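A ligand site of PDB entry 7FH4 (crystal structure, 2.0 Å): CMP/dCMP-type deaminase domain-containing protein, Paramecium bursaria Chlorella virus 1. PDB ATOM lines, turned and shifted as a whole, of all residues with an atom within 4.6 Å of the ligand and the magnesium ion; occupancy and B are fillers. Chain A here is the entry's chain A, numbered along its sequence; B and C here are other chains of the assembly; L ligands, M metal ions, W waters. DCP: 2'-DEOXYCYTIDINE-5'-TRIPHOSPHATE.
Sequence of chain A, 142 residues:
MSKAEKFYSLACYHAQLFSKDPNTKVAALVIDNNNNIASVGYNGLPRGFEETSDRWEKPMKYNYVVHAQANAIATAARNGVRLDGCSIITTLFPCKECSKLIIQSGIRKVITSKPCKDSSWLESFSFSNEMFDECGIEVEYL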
ATOM      1  N   LYS A  20     -24.965  29.382  25.838  1.00  0.00           N
ATOM      2  CA  LYS A  20     -25.803  29.922  26.906  1.00  0.00           C
ATOM      3  C   LYS A  20     -24.998  30.584  28.018  1.00  0.00           C
ATOM      4  O   LYS A  20     -25.578  31.000  29.015  1.00  0.00           O
ATOM      5  CB  LYS A  20     -26.680  28.802  27.509  1.00  0.00           C
ATOM      6  CG  LYS A  20     -27.593  28.066  26.515  1.00  0.00           C
ATOM      7  CD  LYS A  20     -28.736  27.328  27.263  1.00  0.00           C
ATOM      8  CE  LYS A  20     -29.381  26.223  26.415  1.00  0.00           C
ATOM      9  NZ  LYS A  20     -28.364  25.234  25.899  1.00  0.00           N
ATOM     10  N   VAL A  40     -16.522  21.180  15.083  1.00  0.00           N
ATOM     11  CA  VAL A  40     -17.055  22.454  15.560  1.00  0.00           C
ATOM     12  C   VAL A  40     -17.493  22.273  16.999  1.00  0.00           C
ATOM     13  O   VAL A  40     -18.039  21.222  17.356  1.00  0.00           O
ATOM     14  CB  VAL A  40     -18.249  22.944  14.695  1.00  0.00           C
ATOM     15  CG1 VAL A  40     -18.583  24.371  15.045  1.00  0.00           C
ATOM     16  CG2 VAL A  40     -17.956  22.805  13.198  1.00  0.00           C
ATOM     17  N   GLY A  41     -17.260  23.287  17.821  1.00  0.00           N
ATOM     18  CA  GLY A  41     -17.757  23.257  19.195  1.00  0.00           C
ATOM     19  C   GLY A  41     -18.066  24.643  19.708  1.00  0.00           C
ATOM     20  O   GLY A  41     -17.592  25.653  19.167  1.00  0.00           O
ATOM     21  N   TYR A  42     -18.876  24.690  20.758  1.00  0.00           N
ATOM     22  CA  TYR A  42     -19.114  25.915  21.517  1.00  0.00           C
ATOM     23  C   TYR A  42     -19.117  25.571  23.002  1.00  0.00           C
ATOM     24  O   TYR A  42     -19.217  24.407  23.392  1.00  0.00           O
ATOM     25  CB  TYR A  42     -20.420  26.624  21.105  1.00  0.00           C
ATOM     26  CG  TYR A  42     -21.710  25.809  21.206  1.00  0.00           C
ATOM     27  CD1 TYR A  42     -22.170  25.070  20.115  1.00  0.00           C
ATOM     28  CD2 TYR A  42     -22.487  25.823  22.362  1.00  0.00           C
ATOM     29  CE1 TYR A  42     -23.352  24.330  20.183  1.00  0.00           C
ATOM     30  CE2 TYR A  42     -23.678  25.080  22.435  1.00  0.00           C
ATOM     31  CZ  TYR A  42     -24.093  24.340  21.338  1.00  0.00           C
ATOM     32  OH  TYR A  42     -25.264  23.632  21.382  1.00  0.00           O
ATOM     33  N   GLY A  44     -20.549  25.198  26.712  1.00  0.00           N
ATOM     34  CA  GLY A  44     -21.848  24.928  27.313  1.00  0.00           C
ATOM     35  C   GLY A  44     -21.714  23.844  28.373  1.00  0.00           C
ATOM     36  O   GLY A  44     -20.673  23.181  28.488  1.00  0.00           O
ATOM     37  N   LEU A  45     -22.777  23.692  29.154  1.00  0.00           N
ATOM     38  CA  LEU A  45     -22.802  22.595  30.121  1.00  0.00           C
ATOM     39  C   LEU A  45     -22.897  21.274  29.354  1.00  0.00           C
ATOM     40  O   LEU A  45     -23.275  21.264  28.180  1.00  0.00           O
ATOM     41  CB  LEU A  45     -23.982  22.767  31.081  1.00  0.00           C
ATOM     42  CG  LEU A  45     -24.015  24.121  31.816  1.00  0.00           C
ATOM     43  CD1 LEU A  45     -24.860  24.062  33.073  1.00  0.00           C
ATOM     44  CD2 LEU A  45     -22.623  24.648  32.173  1.00  0.00           C
ATOM     45  N   PRO A  46     -22.531  20.146  29.965  1.00  0.00           N
ATOM     46  CA  PRO A  46     -22.562  18.890  29.217  1.00  0.00           C
ATOM     47  C   PRO A  46     -23.987  18.588  28.738  1.00  0.00           C
ATOM     48  O   PRO A  46     -24.971  19.107  29.268  1.00  0.00           O
ATOM     49  CB  PRO A  46     -22.060  17.855  30.215  1.00  0.00           C
ATOM     50  CG  PRO A  46     -21.294  18.654  31.245  1.00  0.00           C
ATOM     51  CD  PRO A  46     -22.053  19.936  31.348  1.00  0.00           C
ATOM     52  N   ARG A  47     -24.077  17.803  27.667  1.00  0.00           N
ATOM     53  CA  ARG A  47     -25.359  17.533  27.032  1.00  0.00           C
ATOM     54  C   ARG A  47     -26.319  16.851  28.000  1.00  0.00           C
ATOM     55  O   ARG A  47     -25.995  15.820  28.595  1.00  0.00           O
ATOM     56  CB  ARG A  47     -25.155  16.648  25.806  1.00  0.00           C
ATOM     57  CG  ARG A  47     -26.404  16.178  25.101  1.00  0.00           C
ATOM     58  CD  ARG A  47     -26.036  15.340  23.868  1.00  0.00           C
ATOM     59  NE  ARG A  47     -25.518  16.167  22.769  1.00  0.00           N
ATOM     60  CZ  ARG A  47     -24.232  16.394  22.512  1.00  0.00           C
ATOM     61  NH1 ARG A  47     -23.275  15.885  23.287  1.00  0.00           N
ATOM     62  NH2 ARG A  47     -23.898  17.153  21.488  1.00  0.00           N
ATOM     63  N   GLY A  48     -27.510  17.432  28.139  1.00  0.00           N
ATOM     64  CA  GLY A  48     -28.508  16.894  29.032  1.00  0.00           C
ATOM     65  C   GLY A  48     -28.374  17.322  30.469  1.00  0.00           C
ATOM     66  O   GLY A  48     -29.265  17.033  31.265  1.00  0.00           O
ATOM     67  N   PHE A  49     -27.282  17.984  30.832  1.00  0.00           N
ATOM     68  CA  PHE A  49     -27.134  18.503  32.189  1.00  0.00           C
ATOM     69  C   PHE A  49     -28.064  19.706  32.362  1.00  0.00           C
ATOM     70  O   PHE A  49     -28.062  20.619  31.532  1.00  0.00           O
ATOM     71  CB  PHE A  49     -25.675  18.874  32.426  1.00  0.00           C
ATOM     72  CG  PHE A  49     -25.328  19.080  33.872  1.00  0.00           C
ATOM     73  CD1 PHE A  49     -25.447  18.047  34.780  1.00  0.00           C
ATOM     74  CD2 PHE A  49     -24.858  20.298  34.313  1.00  0.00           C
ATOM     75  CE1 PHE A  49     -25.118  18.232  36.107  1.00  0.00           C
ATOM     76  CE2 PHE A  49     -24.507  20.482  35.638  1.00  0.00           C
ATOM     77  CZ  PHE A  49     -24.647  19.449  36.524  1.00  0.00           C
ATOM     78  N   GLU A  51     -29.581  23.086  32.981  1.00  0.00           N
ATOM     79  CA  GLU A  51     -28.926  24.395  32.957  1.00  0.00           C
ATOM     80  C   GLU A  51     -29.737  25.392  33.786  1.00  0.00           C
ATOM     81  O   GLU A  51     -30.679  26.005  33.282  1.00  0.00           O
ATOM     82  CB  GLU A  51     -28.761  24.871  31.515  1.00  0.00           C
ATOM     83  CG  GLU A  51     -28.012  23.855  30.657  1.00  0.00           C
ATOM     84  CD  GLU A  51     -27.495  24.431  29.355  1.00  0.00           C
ATOM     85  OE1 GLU A  51     -26.816  25.491  29.384  1.00  0.00           O
ATOM     86  OE2 GLU A  51     -27.774  23.807  28.305  1.00  0.00           O
ATOM     87  N   VAL A  66     -18.162  23.035  29.667  1.00  0.00           N
ATOM     88  CA  VAL A  66     -17.227  22.432  28.720  1.00  0.00           C
ATOM     89  C   VAL A  66     -16.802  23.526  27.750  1.00  0.00           C
ATOM     90  O   VAL A  66     -17.655  24.213  27.168  1.00  0.00           O
ATOM     91  CB  VAL A  66     -17.851  21.250  27.963  1.00  0.00           C
ATOM     92  CG1 VAL A  66     -16.772  20.515  27.191  1.00  0.00           C
ATOM     93  CG2 VAL A  66     -18.612  20.325  28.942  1.00  0.00           C
ATOM     94  N   ASN A  71     -14.810  20.740  23.354  1.00  0.00           N
ATOM     95  CA  ASN A  71     -15.975  20.125  22.718  1.00  0.00           C
ATOM     96  C   ASN A  71     -15.704  19.759  21.266  1.00  0.00           C
ATOM     97  O   ASN A  71     -16.138  18.699  20.804  1.00  0.00           O
ATOM     98  CB  ASN A  71     -17.188  21.056  22.792  1.00  0.00           C
ATOM     99  CG  ASN A  71     -18.147  20.692  23.938  1.00  0.00           C
ATOM    100  OD1 ASN A  71     -18.332  19.523  24.257  1.00  0.00           O
ATOM    101  ND2 ASN A  71     -18.743  21.698  24.545  1.00  0.00           N
ATOM    102  N   LYS B   3     -32.994  24.690  17.681  1.00  0.00           N
ATOM    103  CA  LYS B   3     -31.663  24.300  17.195  1.00  0.00           C
ATOM    104  C   LYS B   3     -31.604  24.336  15.678  1.00  0.00           C
ATOM    105  O   LYS B   3     -30.677  24.921  15.098  1.00  0.00           O
ATOM    106  CB  LYS B   3     -31.256  22.909  17.693  1.00  0.00           C
ATOM    107  CG  LYS B   3     -31.051  22.810  19.208  1.00  0.00           C
ATOM    108  CD  LYS B   3     -29.882  23.680  19.669  1.00  0.00           C
ATOM    109  CE  LYS B   3     -29.839  23.830  21.186  1.00  0.00           C
ATOM    110  NZ  LYS B   3     -29.539  22.530  21.869  1.00  0.00           N
ATOM    111  N   PHE B   7     -29.118  26.617  13.344  1.00  0.00           N
ATOM    112  CA  PHE B   7     -28.226  26.092  12.309  1.00  0.00           C
ATOM    113  C   PHE B   7     -28.535  26.716  10.961  1.00  0.00           C
ATOM    114  O   PHE B   7     -27.622  27.035  10.190  1.00  0.00           O
ATOM    115  CB  PHE B   7     -28.335  24.570  12.213  1.00  0.00           C
ATOM    116  CG  PHE B   7     -27.609  23.825  13.293  1.00  0.00           C
ATOM    117  CD1 PHE B   7     -26.244  23.969  13.459  1.00  0.00           C
ATOM    118  CD2 PHE B   7     -28.304  22.949  14.116  1.00  0.00           C
ATOM    119  CE1 PHE B   7     -25.568  23.255  14.448  1.00  0.00           C
ATOM    120  CE2 PHE B   7     -27.650  22.236  15.107  1.00  0.00           C
ATOM    121  CZ  PHE B   7     -26.274  22.389  15.277  1.00  0.00           C
ATOM    122  N   ASN B  34     -27.119  13.945  17.536  1.00  0.00           N
ATOM    123  CA  ASN B  34     -26.716  14.691  18.718  1.00  0.00           C
ATOM    124  C   ASN B  34     -26.548  16.174  18.421  1.00  0.00           C
ATOM    125  O   ASN B  34     -25.987  16.906  19.254  1.00  0.00           O
ATOM    126  CB  ASN B  34     -25.407  14.105  19.275  1.00  0.00           C
ATOM    127  CG  ASN B  34     -25.563  12.644  19.678  1.00  0.00           C
ATOM    128  OD1 ASN B  34     -26.484  12.284  20.393  1.00  0.00           O
ATOM    129  ND2 ASN B  34     -24.647  11.797  19.211  1.00  0.00           N
ATOM    130  N   ASN B  35     -27.006  16.630  17.254  1.00  0.00           N
ATOM    131  CA  ASN B  35     -26.835  18.000  16.779  1.00  0.00           C
ATOM    132  C   ASN B  35     -25.368  18.378  16.598  1.00  0.00           C
ATOM    133  O   ASN B  35     -25.028  19.567  16.618  1.00  0.00           O
ATOM    134  CB  ASN B  35     -27.547  19.005  17.688  1.00  0.00           C
ATOM    135  CG  ASN B  35     -29.061  19.014  17.468  1.00  0.00           C
ATOM    136  OD1 ASN B  35     -29.538  18.843  16.351  1.00  0.00           O
ATOM    137  ND2 ASN B  35     -29.808  19.223  18.540  1.00  0.00           N
ATOM    138  N   ASN B  36     -24.502  17.401  16.420  1.00  0.00           N
ATOM    139  CA  ASN B  36     -23.128  17.713  16.039  1.00  0.00           C
ATOM    140  C   ASN B  36     -23.014  17.835  14.538  1.00  0.00           C
ATOM    141  O   ASN B  36     -23.706  17.156  13.771  1.00  0.00           O
ATOM    142  CB  ASN B  36     -22.151  16.661  16.559  1.00  0.00           C
ATOM    143  CG  ASN B  36     -21.803  16.890  18.001  1.00  0.00           C
ATOM    144  OD1 ASN B  36     -21.565  18.028  18.420  1.00  0.00           O
ATOM    145  ND2 ASN B  36     -21.798  15.817  18.784  1.00  0.00           N
ATOM    146  N   ILE B  37     -22.118  18.728  14.111  1.00  0.00           N
ATOM    147  CA  ILE B  37     -21.906  19.028  12.704  1.00  0.00           C
ATOM    148  C   ILE B  37     -20.948  17.995  12.116  1.00  0.00           C
ATOM    149  O   ILE B  37     -19.808  17.847  12.578  1.00  0.00           O
ATOM    150  CB  ILE B  37     -21.373  20.449  12.514  1.00  0.00           C
ATOM    151  CG1 ILE B  37     -22.438  21.468  12.915  1.00  0.00           C
ATOM    152  CG2 ILE B  37     -20.918  20.678  11.050  1.00  0.00           C
ATOM    153  CD1 ILE B  37     -21.890  22.861  13.067  1.00  0.00           C
ATOM    154  N   GLN C 104     -19.108  14.181  26.782  1.00  0.00           N
ATOM    155  CA  GLN C 104     -19.209  14.735  25.432  1.00  0.00           C
ATOM    156  C   GLN C 104     -18.689  13.786  24.359  1.00  0.00           C
ATOM    157  O   GLN C 104     -19.097  13.900  23.198  1.00  0.00           O
ATOM    158  CB  GLN C 104     -18.481  16.067  25.330  1.00  0.00           C
ATOM    159  CG  GLN C 104     -19.144  17.171  26.198  1.00  0.00           C
ATOM    160  CD  GLN C 104     -20.597  17.437  25.832  1.00  0.00           C
ATOM    161  OE1 GLN C 104     -21.503  17.200  26.641  1.00  0.00           O
ATOM    162  NE2 GLN C 104     -20.824  17.936  24.627  1.00  0.00           N
HETATM  163  N1  DCP L   1     -22.310  21.019  21.722  1.00  0.00           N
HETATM  164  C2  DCP L   1     -21.359  21.468  20.801  1.00  0.00           C
HETATM  165  N3  DCP L   1     -21.687  21.507  19.485  1.00  0.00           N
HETATM  166  C4  DCP L   1     -22.904  21.131  19.081  1.00  0.00           C
HETATM  167  C5  DCP L   1     -23.885  20.678  20.009  1.00  0.00           C
HETATM  168  C6  DCP L   1     -23.542  20.634  21.301  1.00  0.00           C
HETATM  169  O2  DCP L   1     -20.237  21.808  21.220  1.00  0.00           O
HETATM  170  N4  DCP L   1     -23.167  21.192  17.777  1.00  0.00           N
HETATM  171  C1' DCP L   1     -21.947  20.977  23.147  1.00  0.00           C
HETATM  172  C2' DCP L   1     -22.134  22.289  23.885  1.00  0.00           C
HETATM  173  C3' DCP L   1     -22.432  21.835  25.304  1.00  0.00           C
HETATM  174  C4' DCP L   1     -23.194  20.525  25.096  1.00  0.00           C
HETATM  175  O4' DCP L   1     -22.799  20.044  23.785  1.00  0.00           O
HETATM  176  O3' DCP L   1     -21.223  21.597  26.021  1.00  0.00           O
HETATM  177  C5' DCP L   1     -24.700  20.640  25.158  1.00  0.00           C
HETATM  178  O5' DCP L   1     -25.144  21.671  24.243  1.00  0.00           O
HETATM  179  PA  DCP L   1     -26.578  22.341  24.488  1.00  0.00           P
HETATM  180  O1A DCP L   1     -26.780  23.441  23.501  1.00  0.00           O
HETATM  181  O2A DCP L   1     -26.729  22.664  25.942  1.00  0.00           O
HETATM  182  O3A DCP L   1     -27.556  21.130  24.124  1.00  0.00           O
HETATM  183  PB  DCP L   1     -28.344  20.068  25.021  1.00  0.00           P
HETATM  184  O1B DCP L   1     -27.814  20.126  26.413  1.00  0.00           O
HETATM  185  O2B DCP L   1     -28.384  18.767  24.295  1.00  0.00           O
HETATM  186  O3B DCP L   1     -29.817  20.703  24.999  1.00  0.00           O
HETATM  187  PG  DCP L   1     -30.419  22.073  25.589  1.00  0.00           P
HETATM  188  O1G DCP L   1     -30.071  23.148  24.582  1.00  0.00           O
HETATM  189  O2G DCP L   1     -29.746  22.291  26.919  1.00  0.00           O
HETATM  190  O3G DCP L   1     -31.904  21.862  25.712  1.00  0.00           O
HETATM  191 MG    MG M   1     -27.807  21.867  27.459  1.00  0.00          MG
HETATM  192  O   HOH W   1     -27.586  21.082  20.650  1.00  0.00           O
HETATM  193  O   HOH W   2     -27.036  18.586  21.848  1.00  0.00           O
HETATM  194  O   HOH W   3     -26.084  21.369  28.518  1.00  0.00           O
HETATM  195  O   HOH W   4     -27.248  25.976  23.396  1.00  0.00           O
HETATM  196  O   HOH W   5     -31.789  24.973  23.799  1.00  0.00           O
HETATM  197  O   HOH W   6     -30.443  17.863  22.923  1.00  0.00           O
HETATM  198  O   HOH W   7     -18.761  19.892  19.474  1.00  0.00           O
HETATM  199  O   HOH W   8     -20.609  19.885  16.322  1.00  0.00           O
HETATM  200  O   HOH W   9     -21.189  18.344  20.978  1.00  0.00           O
HETATM  201  O   HOH W  10     -28.770  20.629  28.994  1.00  0.00           O
HETATM  202  O   HOH W  11     -31.230  23.873  28.511  1.00  0.00           O
HETATM  203  O   HOH W  12     -25.051  24.525  27.316  1.00  0.00           O
HETATM  204  O   HOH W  13     -20.659  23.060  17.535  1.00  0.00           O
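The magnesium ion is bound by O2A of the ligand (2.0 Å), O1B of the ligand (2.0 Å), O2G of the ligand (2.1 Å), water W3 (2.1 Å), OE2 of Glu 51 (2.1 Å) and water W10 (2.2 Å). The magnesium ion has six donor atoms within binding distance.
The backbone carbonyl oxygen of Asn 35 of chain B is in hydrogen-bond range of a nitrogen (N4) of the ligand (2.7 Å). The backbone carbonyl oxygen of Gly 44 lies within hydrogen-bond range of an oxygen (O3') of the ligand (3.0 Å). The side-chain amino group (NZ) of Lys 3 of chain B is in salt-bridge range of an oxygen (O1G) of the ligand (2.8 Å). An oxygen (O4') of the ligand is in hydrogen-bond range of the side-chain amide nitrogen (NE2) of Gln 104 of chain C, 3.0 Å away. An oxygen (O1B) of the ligand sits close to the backbone NH (N) of Gly 48 (3.2 Å). The backbone NH of Tyr 42 is in hydrogen-bond range of an oxygen (O2) of the ligand. The side-chain hydroxyl (OH) of Tyr 42 lies within hydrogen-bond range of an oxygen (O1A) of the ligand, at 2.6 Å. NZ of Lys 20 lies within salt-bridge range of O1G of the ligand, at 3.0 Å. The side-chain amide nitrogen (ND2) of Asn 71 sits at hydrogen-bond distance from an oxygen (O3') of the ligand (2.9 Å). O of Leu 45 lies within hydrogen-bond range of O3' of the ligand (3.0 Å).
Residues that only touch the ligand: Gly 41 (3.5 Å), Arg 47 (3.4 Å), Val 66 (3.9 Å) and Asn 36 of chain B (3.4 Å). 14 residues have an atom within 4 Å of the ligand: Lys 20, Gly 41, Tyr 42, Gly 44, Leu 45, Arg 47, Gly 48, Glu 51, Val 66, Asn 71, Lys 3 of chain B, Asn 35 of chain B, Asn 36 of chain B and Gln 104 of chain C. The nearest printed residue that does not touch the ligand is Pro 46 (4.2 Å).
The backbone carbonyl oxygen of Gly 44 is in hydrogen-bond range of the backbone NH of Val 66, 2.8 Å away. The side-chain amide nitrogen (NE2) of Gln 104 of chain C sits at hydrogen-bond distance from the side-chain amide oxygen (OD1) of Asn 71 (3.0 Å). The backbone NH (N) of Arg 47 lies within hydrogen-bond range of the side-chain amide oxygen (OE1) of Gln 104 of chain C (2.8 Å). The backbone carbonyl oxygen (O) of Asn 34 of chain B lies within hydrogen-bond range of the guanidinium group (NH2) of Arg 47, at 3.1 Å. The side-chain carboxylate of Glu 51 lies within salt-bridge range of the side-chain amino group of Lys 20 (3.8 Å). The backbone carbonyl oxygen (O) of Tyr 42 sits at hydrogen-bond distance from the side-chain amide nitrogen (ND2) of Asn 71, at 3.0 Å.
Water W4 bridges an oxygen (O1A) of the ligand (2.6 Å) and the side-chain amino group (NZ) of Lys 20 (2.8 Å). Water W13 lies within hydrogen-bond range of a nitrogen (N3) of the ligand (2.7 Å), the backbone carbonyl oxygen of Val 40 (3.2 Å) and the backbone NH of Gly 41 (3.4 Å). Water W2 lies within hydrogen-bond range of O2B of the ligand, NE of Arg 47 and O of Asn 34 of chain B. Water W12 lies within hydrogen-bond range of OE1 of Glu 51 (2.9 Å) and N of Leu 45 (3.0 Å). Water W8 lies within hydrogen-bond range of the backbone NH of Ile 37 of chain B (2.9 Å), the side-chain amide oxygen of Asn 36 of chain B (3.0 Å), the backbone carbonyl oxygen of Val 40 (3.1 Å) and a nitrogen (N4) of the ligand (3.2 Å). Water W1 bridges NZ of Lys 3 of chain B (2.7 Å) and O3A of the ligand (3.5 Å).
Residues that only touch the magnesium ion: Lys 20. Two residues have an atom within 4 Å of the magnesium ion: Lys 20 and Glu 51.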
